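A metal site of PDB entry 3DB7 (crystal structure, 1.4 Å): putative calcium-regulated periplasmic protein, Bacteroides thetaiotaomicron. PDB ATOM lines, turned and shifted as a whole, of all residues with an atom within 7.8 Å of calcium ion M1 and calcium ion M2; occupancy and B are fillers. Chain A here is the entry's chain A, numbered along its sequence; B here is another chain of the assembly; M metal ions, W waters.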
ATOM      1  N   ASP A   5     -25.038  13.000  -8.423  1.00  0.00           N
ATOM      2  CA  ASP A   5     -24.272  12.284  -9.459  1.00  0.00           C
ATOM      3  C   ASP A   5     -25.187  11.283 -10.144  1.00  0.00           C
ATOM      4  O   ASP A   5     -25.925  10.540  -9.491  1.00  0.00           O
ATOM      5  CB  ASP A   5     -23.102  11.488  -8.852  1.00  0.00           C
ATOM      6  CG  ASP A   5     -21.876  12.333  -8.530  1.00  0.00           C
ATOM      7  OD1 ASP A   5     -21.825  13.579  -8.765  1.00  0.00           O
ATOM      8  OD2 ASP A   5     -20.908  11.716  -8.015  1.00  0.00           O
ATOM      9  N   LYS A  34     -20.379   9.639 -15.703  1.00  0.00           N
ATOM     10  CA  LYS A  34     -21.470  10.239 -14.946  1.00  0.00           C
ATOM     11  C   LYS A  34     -21.724  11.682 -15.399  1.00  0.00           C
ATOM     12  O   LYS A  34     -20.841  12.355 -15.878  1.00  0.00           O
ATOM     13  CB  LYS A  34     -21.212  10.209 -13.446  1.00  0.00           C
ATOM     14  CG  LYS A  34     -20.150  11.168 -12.994  1.00  0.00           C
ATOM     15  CD  LYS A  34     -19.938  11.136 -11.473  1.00  0.00           C
ATOM     16  CE  LYS A  34     -19.073  12.321 -10.997  1.00  0.00           C
ATOM     17  NZ  LYS A  34     -18.581  12.101  -9.585  1.00  0.00           N
ATOM     18  N   GLU A  36     -22.484  15.136 -13.612  1.00  0.00           N
ATOM     19  CA  GLU A  36     -22.218  15.828 -12.341  1.00  0.00           C
ATOM     20  C   GLU A  36     -22.979  17.133 -12.413  1.00  0.00           C
ATOM     21  O   GLU A  36     -23.004  17.788 -13.446  1.00  0.00           O
ATOM     22  CB  GLU A  36     -20.735  16.004 -12.157  1.00  0.00           C
ATOM     23  CG  GLU A  36     -20.327  16.751 -10.892  1.00  0.00           C
ATOM     24  CD  GLU A  36     -18.837  17.074 -10.863  1.00  0.00           C
ATOM     25  OE1 GLU A  36     -18.061  16.153 -11.126  1.00  0.00           O
ATOM     26  OE2 GLU A  36     -18.468  18.249 -10.602  1.00  0.00           O
ATOM     27  N   SER A  37     -23.652  17.504 -11.344  1.00  0.00           N
ATOM     28  CA  SER A  37     -24.436  18.732 -11.412  1.00  0.00           C
ATOM     29  C   SER A  37     -24.729  19.300 -10.052  1.00  0.00           C
ATOM     30  O   SER A  37     -24.596  18.600  -9.024  1.00  0.00           O
ATOM     31  CB  SER A  37     -25.746  18.531 -12.191  1.00  0.00           C
ATOM     32  OG  SER A  37     -26.597  17.685 -11.445  1.00  0.00           O
ATOM     33  N   TYR A  41     -24.672  24.318 -12.380  1.00  0.00           N
ATOM     34  CA  TYR A  41     -23.819  23.728 -13.402  1.00  0.00           C
ATOM     35  C   TYR A  41     -24.193  22.292 -13.672  1.00  0.00           C
ATOM     36  O   TYR A  41     -24.840  21.629 -12.894  1.00  0.00           O
ATOM     37  CB  TYR A  41     -22.382  23.823 -13.025  1.00  0.00           C
ATOM     38  CG  TYR A  41     -21.870  22.717 -12.106  1.00  0.00           C
ATOM     39  CD1 TYR A  41     -22.030  22.760 -10.723  1.00  0.00           C
ATOM     40  CD2 TYR A  41     -21.183  21.641 -12.620  1.00  0.00           C
ATOM     41  CE1 TYR A  41     -21.505  21.770  -9.886  1.00  0.00           C
ATOM     42  CE2 TYR A  41     -20.676  20.640 -11.805  1.00  0.00           C
ATOM     43  CZ  TYR A  41     -20.793  20.729 -10.408  1.00  0.00           C
ATOM     44  OH  TYR A  41     -20.244  19.755  -9.525  1.00  0.00           O
ATOM     45  N   SER A  43     -21.835  19.044 -15.663  1.00  0.00           N
ATOM     46  CA  SER A  43     -20.660  18.554 -16.367  1.00  0.00           C
ATOM     47  C   SER A  43     -20.733  17.065 -16.483  1.00  0.00           C
ATOM     48  O   SER A  43     -21.628  16.427 -15.956  1.00  0.00           O
ATOM     49  CB  SER A  43     -19.361  18.908 -15.648  1.00  0.00           C
ATOM     50  OG  SER A  43     -19.404  18.338 -14.366  1.00  0.00           O
ATOM     51  N   TYR A  44     -19.766  16.494 -17.221  1.00  0.00           N
ATOM     52  CA  TYR A  44     -19.694  15.075 -17.452  1.00  0.00           C
ATOM     53  C   TYR A  44     -18.327  14.614 -17.074  1.00  0.00           C
ATOM     54  O   TYR A  44     -17.337  15.170 -17.549  1.00  0.00           O
ATOM     55  CB  TYR A  44     -19.957  14.767 -18.938  1.00  0.00           C
ATOM     56  CG  TYR A  44     -21.337  15.098 -19.386  1.00  0.00           C
ATOM     57  CD1 TYR A  44     -22.406  14.235 -19.204  1.00  0.00           C
ATOM     58  CD2 TYR A  44     -21.598  16.323 -19.971  1.00  0.00           C
ATOM     59  CE1 TYR A  44     -23.674  14.572 -19.622  1.00  0.00           C
ATOM     60  CE2 TYR A  44     -22.866  16.698 -20.350  1.00  0.00           C
ATOM     61  CZ  TYR A  44     -23.884  15.829 -20.184  1.00  0.00           C
ATOM     62  OH  TYR A  44     -25.157  16.215 -20.604  1.00  0.00           O
ATOM     63  N   GLU A  45     -18.197  13.523 -16.315  1.00  0.00           N
ATOM     64  CA  GLU A  45     -16.907  12.957 -15.968  1.00  0.00           C
ATOM     65  C   GLU A  45     -16.857  11.523 -16.459  1.00  0.00           C
ATOM     66  O   GLU A  45     -17.822  10.759 -16.347  1.00  0.00           O
ATOM     67  CB  GLU A  45     -16.659  12.963 -14.443  1.00  0.00           C
ATOM     68  CG  GLU A  45     -16.404  14.336 -13.771  1.00  0.00           C
ATOM     69  CD  GLU A  45     -15.857  14.276 -12.368  1.00  0.00           C
ATOM     70  OE1 GLU A  45     -15.978  13.271 -11.651  1.00  0.00           O
ATOM     71  OE2 GLU A  45     -15.326  15.317 -11.946  1.00  0.00           O
ATOM     72  N   LYS A  53      -8.981  10.407 -15.505  1.00  0.00           N
ATOM     73  CA  LYS A  53     -10.301  11.018 -15.619  1.00  0.00           C
ATOM     74  C   LYS A  53     -10.286  12.182 -16.574  1.00  0.00           C
ATOM     75  O   LYS A  53      -9.304  12.953 -16.627  1.00  0.00           O
ATOM     76  CB  LYS A  53     -10.778  11.522 -14.226  1.00  0.00           C
ATOM     77  CG  LYS A  53     -12.222  11.967 -14.189  1.00  0.00           C
ATOM     78  CD  LYS A  53     -12.537  12.823 -12.963  1.00  0.00           C
ATOM     79  CE  LYS A  53     -12.115  14.265 -13.135  1.00  0.00           C
ATOM     80  NZ  LYS A  53     -12.471  15.172 -11.999  1.00  0.00           N
ATOM     81  N   VAL A  54     -11.387  12.347 -17.264  1.00  0.00           N
ATOM     82  CA  VAL A  54     -11.618  13.565 -18.018  1.00  0.00           C
ATOM     83  C   VAL A  54     -12.950  14.146 -17.614  1.00  0.00           C
ATOM     84  O   VAL A  54     -13.930  13.406 -17.427  1.00  0.00           O
ATOM     85  CB  VAL A  54     -11.665  13.346 -19.551  1.00  0.00           C
ATOM     86  CG1 VAL A  54     -11.887  14.664 -20.302  1.00  0.00           C
ATOM     87  CG2 VAL A  54     -10.334  12.711 -20.022  1.00  0.00           C
ATOM     88  N   GLU A  55     -13.019  15.465 -17.440  1.00  0.00           N
ATOM     89  CA  GLU A  55     -14.263  16.174 -17.215  1.00  0.00           C
ATOM     90  C   GLU A  55     -14.509  17.117 -18.337  1.00  0.00           C
ATOM     91  O   GLU A  55     -13.580  17.792 -18.815  1.00  0.00           O
ATOM     92  CB  GLU A  55     -14.239  16.934 -15.896  1.00  0.00           C
ATOM     93  CG  GLU A  55     -15.602  17.527 -15.528  1.00  0.00           C
ATOM     94  CD  GLU A  55     -15.717  17.840 -14.049  1.00  0.00           C
ATOM     95  OE1 GLU A  55     -14.651  18.000 -13.332  1.00  0.00           O
ATOM     96  OE2 GLU A  55     -16.858  17.915 -13.581  1.00  0.00           O
ATOM     97  N   PHE A  56     -15.769  17.192 -18.739  1.00  0.00           N
ATOM     98  CA  PHE A  56     -16.250  17.982 -19.859  1.00  0.00           C
ATOM     99  C   PHE A  56     -17.334  18.924 -19.410  1.00  0.00           C
ATOM    100  O   PHE A  56     -18.101  18.626 -18.478  1.00  0.00           O
ATOM    101  CB  PHE A  56     -16.840  17.090 -20.964  1.00  0.00           C
ATOM    102  CG  PHE A  56     -15.928  16.009 -21.469  1.00  0.00           C
ATOM    103  CD1 PHE A  56     -15.106  16.258 -22.579  1.00  0.00           C
ATOM    104  CD2 PHE A  56     -15.950  14.730 -20.952  1.00  0.00           C
ATOM    105  CE1 PHE A  56     -14.305  15.262 -23.073  1.00  0.00           C
ATOM    106  CE2 PHE A  56     -15.139  13.719 -21.459  1.00  0.00           C
ATOM    107  CZ  PHE A  56     -14.334  13.995 -22.507  1.00  0.00           C
ATOM    108  N   GLU A  63     -12.632  20.156 -19.937  1.00  0.00           N
ATOM    109  CA  GLU A  63     -12.203  21.181 -18.971  1.00  0.00           C
ATOM    110  C   GLU A  63     -11.099  20.679 -18.039  1.00  0.00           C
ATOM    111  O   GLU A  63     -10.345  21.488 -17.506  1.00  0.00           O
ATOM    112  CB  GLU A  63     -13.368  21.691 -18.137  1.00  0.00           C
ATOM    113  CG  GLU A  63     -14.290  22.603 -18.906  1.00  0.00           C
ATOM    114  CD  GLU A  63     -15.461  23.181 -18.127  1.00  0.00           C
ATOM    115  OE1 GLU A  63     -16.132  22.423 -17.392  1.00  0.00           O
ATOM    116  OE2 GLU A  63     -15.751  24.371 -18.376  1.00  0.00           O
ATOM    117  N   GLU A  64     -10.973  19.339 -17.893  1.00  0.00           N
ATOM    118  CA  GLU A  64      -9.962  18.741 -17.024  1.00  0.00           C
ATOM    119  C   GLU A  64      -9.574  17.444 -17.604  1.00  0.00           C
ATOM    120  O   GLU A  64     -10.436  16.616 -17.910  1.00  0.00           O
ATOM    121  CB  GLU A  64     -10.521  18.535 -15.610  1.00  0.00           C
ATOM    122  CG  GLU A  64      -9.562  17.829 -14.674  1.00  0.00           C
ATOM    123  CD  GLU A  64     -10.213  17.371 -13.343  1.00  0.00           C
ATOM    124  OE1 GLU A  64     -11.421  17.657 -13.067  1.00  0.00           O
ATOM    125  OE2 GLU A  64      -9.487  16.706 -12.582  1.00  0.00           O
ATOM    126  N   VAL A  65      -8.296  17.217 -17.808  1.00  0.00           N
ATOM    127  CA  VAL A  65      -7.756  15.918 -18.174  1.00  0.00           C
ATOM    128  C   VAL A  65      -6.750  15.554 -17.093  1.00  0.00           C
ATOM    129  O   VAL A  65      -5.677  16.174 -17.008  1.00  0.00           O
ATOM    130  CB  VAL A  65      -7.071  15.956 -19.556  1.00  0.00           C
ATOM    131  CG1 VAL A  65      -6.454  14.585 -19.857  1.00  0.00           C
ATOM    132  CG2 VAL A  65      -8.071  16.366 -20.633  1.00  0.00           C
ATOM    133  N   LYS A  96      -1.699  16.574 -15.324  1.00  0.00           N
ATOM    134  CA  LYS A  96      -3.039  17.101 -15.452  1.00  0.00           C
ATOM    135  C   LYS A  96      -2.993  18.403 -16.210  1.00  0.00           C
ATOM    136  O   LYS A  96      -2.017  19.143 -16.116  1.00  0.00           O
ATOM    137  CB  LYS A  96      -3.660  17.343 -14.063  1.00  0.00           C
ATOM    138  CG  LYS A  96      -5.074  17.894 -14.098  1.00  0.00           C
ATOM    139  CD  LYS A  96      -5.711  17.817 -12.741  1.00  0.00           C
ATOM    140  CE  LYS A  96      -4.803  18.460 -11.729  1.00  0.00           C
ATOM    141  NZ  LYS A  96      -5.412  18.354 -10.339  1.00  0.00           N
ATOM    142  N   GLU A  98      -5.946  21.588 -17.129  1.00  0.00           N
ATOM    143  CA  GLU A  98      -7.284  22.164 -16.962  1.00  0.00           C
ATOM    144  C   GLU A  98      -7.376  23.441 -17.714  1.00  0.00           C
ATOM    145  O   GLU A  98      -6.379  24.134 -17.909  1.00  0.00           O
ATOM    146  CB  GLU A  98      -7.545  22.466 -15.509  1.00  0.00           C
ATOM    147  CG  GLU A  98      -7.520  21.219 -14.642  1.00  0.00           C
ATOM    148  CD  GLU A  98      -7.547  21.503 -13.147  1.00  0.00           C
ATOM    149  OE1 GLU A  98      -6.523  21.964 -12.587  1.00  0.00           O
ATOM    150  OE2 GLU A  98      -8.583  21.269 -12.512  1.00  0.00           O
ATOM    151  N   GLU B 113     -11.437  18.488  -4.239  1.00  0.00           N
ATOM    152  CA  GLU B 113     -11.257  19.872  -4.633  1.00  0.00           C
ATOM    153  C   GLU B 113     -12.633  20.405  -5.057  1.00  0.00           C
ATOM    154  O   GLU B 113     -13.340  19.735  -5.796  1.00  0.00           O
ATOM    155  CB  GLU B 113     -10.300  19.997  -5.819  1.00  0.00           C
ATOM    156  CG  GLU B 113      -8.927  19.432  -5.552  1.00  0.00           C
ATOM    157  CD  GLU B 113      -7.933  19.668  -6.721  1.00  0.00           C
ATOM    158  OE1 GLU B 113      -8.236  20.471  -7.650  1.00  0.00           O
ATOM    159  OE2 GLU B 113      -6.826  19.082  -6.678  1.00  0.00           O
ATOM    160  N   LYS B 115     -14.830  23.915  -6.381  1.00  0.00           N
ATOM    161  CA  LYS B 115     -14.766  25.260  -6.983  1.00  0.00           C
ATOM    162  C   LYS B 115     -16.107  25.918  -6.808  1.00  0.00           C
ATOM    163  O   LYS B 115     -17.155  25.296  -6.942  1.00  0.00           O
ATOM    164  CB  LYS B 115     -14.423  25.149  -8.465  1.00  0.00           C
ATOM    165  CG  LYS B 115     -12.990  24.707  -8.699  1.00  0.00           C
ATOM    166  CD  LYS B 115     -12.620  24.533 -10.201  1.00  0.00           C
ATOM    167  CE  LYS B 115     -12.694  25.801 -10.922  1.00  0.00           C
ATOM    168  NZ  LYS B 115     -12.281  25.633 -12.414  1.00  0.00           N
ATOM    169  N   ILE B 123     -19.546  25.114  -8.454  1.00  0.00           N
ATOM    170  CA  ILE B 123     -19.414  24.869  -9.902  1.00  0.00           C
ATOM    171  C   ILE B 123     -18.538  23.671 -10.263  1.00  0.00           C
ATOM    172  O   ILE B 123     -18.466  23.308 -11.438  1.00  0.00           O
ATOM    173  CB  ILE B 123     -18.933  26.130 -10.643  1.00  0.00           C
ATOM    174  CG1 ILE B 123     -17.547  26.595 -10.174  1.00  0.00           C
ATOM    175  CG2 ILE B 123     -20.053  27.272 -10.542  1.00  0.00           C
ATOM    176  CD1 ILE B 123     -16.971  27.759 -10.992  1.00  0.00           C
ATOM    177  N   ASP B 124     -17.944  23.006  -9.267  1.00  0.00           N
ATOM    178  CA  ASP B 124     -17.205  21.762  -9.523  1.00  0.00           C
ATOM    179  C   ASP B 124     -16.914  21.050  -8.219  1.00  0.00           C
ATOM    180  O   ASP B 124     -16.606  21.657  -7.214  1.00  0.00           O
ATOM    181  CB  ASP B 124     -15.888  22.056 -10.207  1.00  0.00           C
ATOM    182  CG  ASP B 124     -15.273  20.852 -10.944  1.00  0.00           C
ATOM    183  OD1 ASP B 124     -15.851  19.745 -10.887  1.00  0.00           O
ATOM    184  OD2 ASP B 124     -14.191  21.108 -11.566  1.00  0.00           O
ATOM    185  N   ILE B 125     -17.047  19.732  -8.236  1.00  0.00           N
ATOM    186  CA  ILE B 125     -16.449  18.849  -7.233  1.00  0.00           C
ATOM    187  C   ILE B 125     -15.592  17.824  -7.958  1.00  0.00           C
ATOM    188  O   ILE B 125     -16.050  17.211  -8.912  1.00  0.00           O
ATOM    189  CB  ILE B 125     -17.497  18.056  -6.465  1.00  0.00           C
ATOM    190  CG1 ILE B 125     -18.510  19.011  -5.786  1.00  0.00           C
ATOM    191  CG2 ILE B 125     -16.802  17.108  -5.405  1.00  0.00           C
ATOM    192  CD1 ILE B 125     -19.538  18.296  -4.889  1.00  0.00           C
ATOM    193  N   ASP B 126     -14.334  17.675  -7.524  1.00  0.00           N
ATOM    194  CA  ASP B 126     -13.426  16.659  -8.048  1.00  0.00           C
ATOM    195  C   ASP B 126     -12.960  15.815  -6.896  1.00  0.00           C
ATOM    196  O   ASP B 126     -12.479  16.333  -5.882  1.00  0.00           O
ATOM    197  CB  ASP B 126     -12.242  17.323  -8.708  1.00  0.00           C
ATOM    198  CG  ASP B 126     -12.623  18.049  -9.987  1.00  0.00           C
ATOM    199  OD1 ASP B 126     -13.605  17.616 -10.649  1.00  0.00           O
ATOM    200  OD2 ASP B 126     -11.946  19.057 -10.322  1.00  0.00           O
ATOM    201  N   ASN B 127     -13.102  14.514  -7.024  1.00  0.00           N
ATOM    202  CA  ASN B 127     -12.647  13.634  -5.984  1.00  0.00           C
ATOM    203  C   ASN B 127     -11.415  12.872  -6.348  1.00  0.00           C
ATOM    204  O   ASN B 127     -10.917  12.922  -7.484  1.00  0.00           O
ATOM    205  CB  ASN B 127     -13.744  12.660  -5.590  1.00  0.00           C
ATOM    206  CG  ASN B 127     -14.977  13.365  -5.123  1.00  0.00           C
ATOM    207  OD1 ASN B 127     -14.916  14.129  -4.157  1.00  0.00           O
ATOM    208  ND2 ASN B 127     -16.095  13.138  -5.791  1.00  0.00           N
ATOM    209  OXT ASN B 127     -10.885  12.159  -5.473  1.00  0.00           O
HETATM  210 CA    CA M   1     -15.977  17.463 -11.276  1.00  0.00          CA
HETATM  211 CA    CA M   2     -12.913  19.302 -12.536  1.00  0.00          CA
HETATM  212  O   HOH W   1     -13.362  20.442 -14.618  1.00  0.00           O
HETATM  213  O   HOH W   2     -11.010  20.854 -12.823  1.00  0.00           O
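Six residues have an atom within 4 Å of calcium ion M1: Glu 36, Glu 45, Glu 55, Asp 124 of chain B, Ile 125 of chain B and Asp 126 of chain B.
Calcium ion M2 is bound by OE1 of Glu 64 (2.3 Å), OE1 of Glu 55 (2.3 Å), water W1 (2.4 Å), OD2 of Asp 124 of chain B (2.4 Å), OD2 of Asp 126 of chain B (2.4 Å), water W2 (2.5 Å) and OD1 of Asp 126 of chain B (2.6 Å).
NZ of Lys 53 lies close to OE1 of Glu 55 (3.8 Å).
The side-chain hydroxyl (OG) of Ser 43 sits close to the side-chain carboxylate (OE2) of Glu 55 (2.7 Å).
OE2 of Glu 45 lies close to NZ of Lys 53 (2.9 Å).
The side-chain amino group (NZ) of Lys 34 lies within salt-bridge range of the side-chain carboxylate (OE1) of Glu 45 (3.5 Å).
OD1 of Asp 126 of chain B lies close to NZ of Lys 53, 3.0 Å away.
N of Asp 126 of chain B is in hydrogen-bond range of O of Glu 113 of chain B (2.9 Å).
N of Ser 43 lies within hydrogen-bond range of O of Glu 36, at 2.8 Å.
The side-chain carboxylate (OE2) of Glu 36 lies close to the side-chain hydroxyl (OH) of Tyr 41, at 2.6 Å.
Calcium ion M1 is bound by OD1 of Asp 124 of chain B (2.3 Å), OE2 of Glu 45 (2.3 Å), O of Ile 125 of chain B (2.4 Å), OD1 of Asp 126 of chain B (2.5 Å), OE1 of Glu 36 (2.5 Å), OE1 of Glu 55 (2.5 Å), OE2 of Glu 55 (2.5 Å) and OE2 of Glu 36 (2.7 Å).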
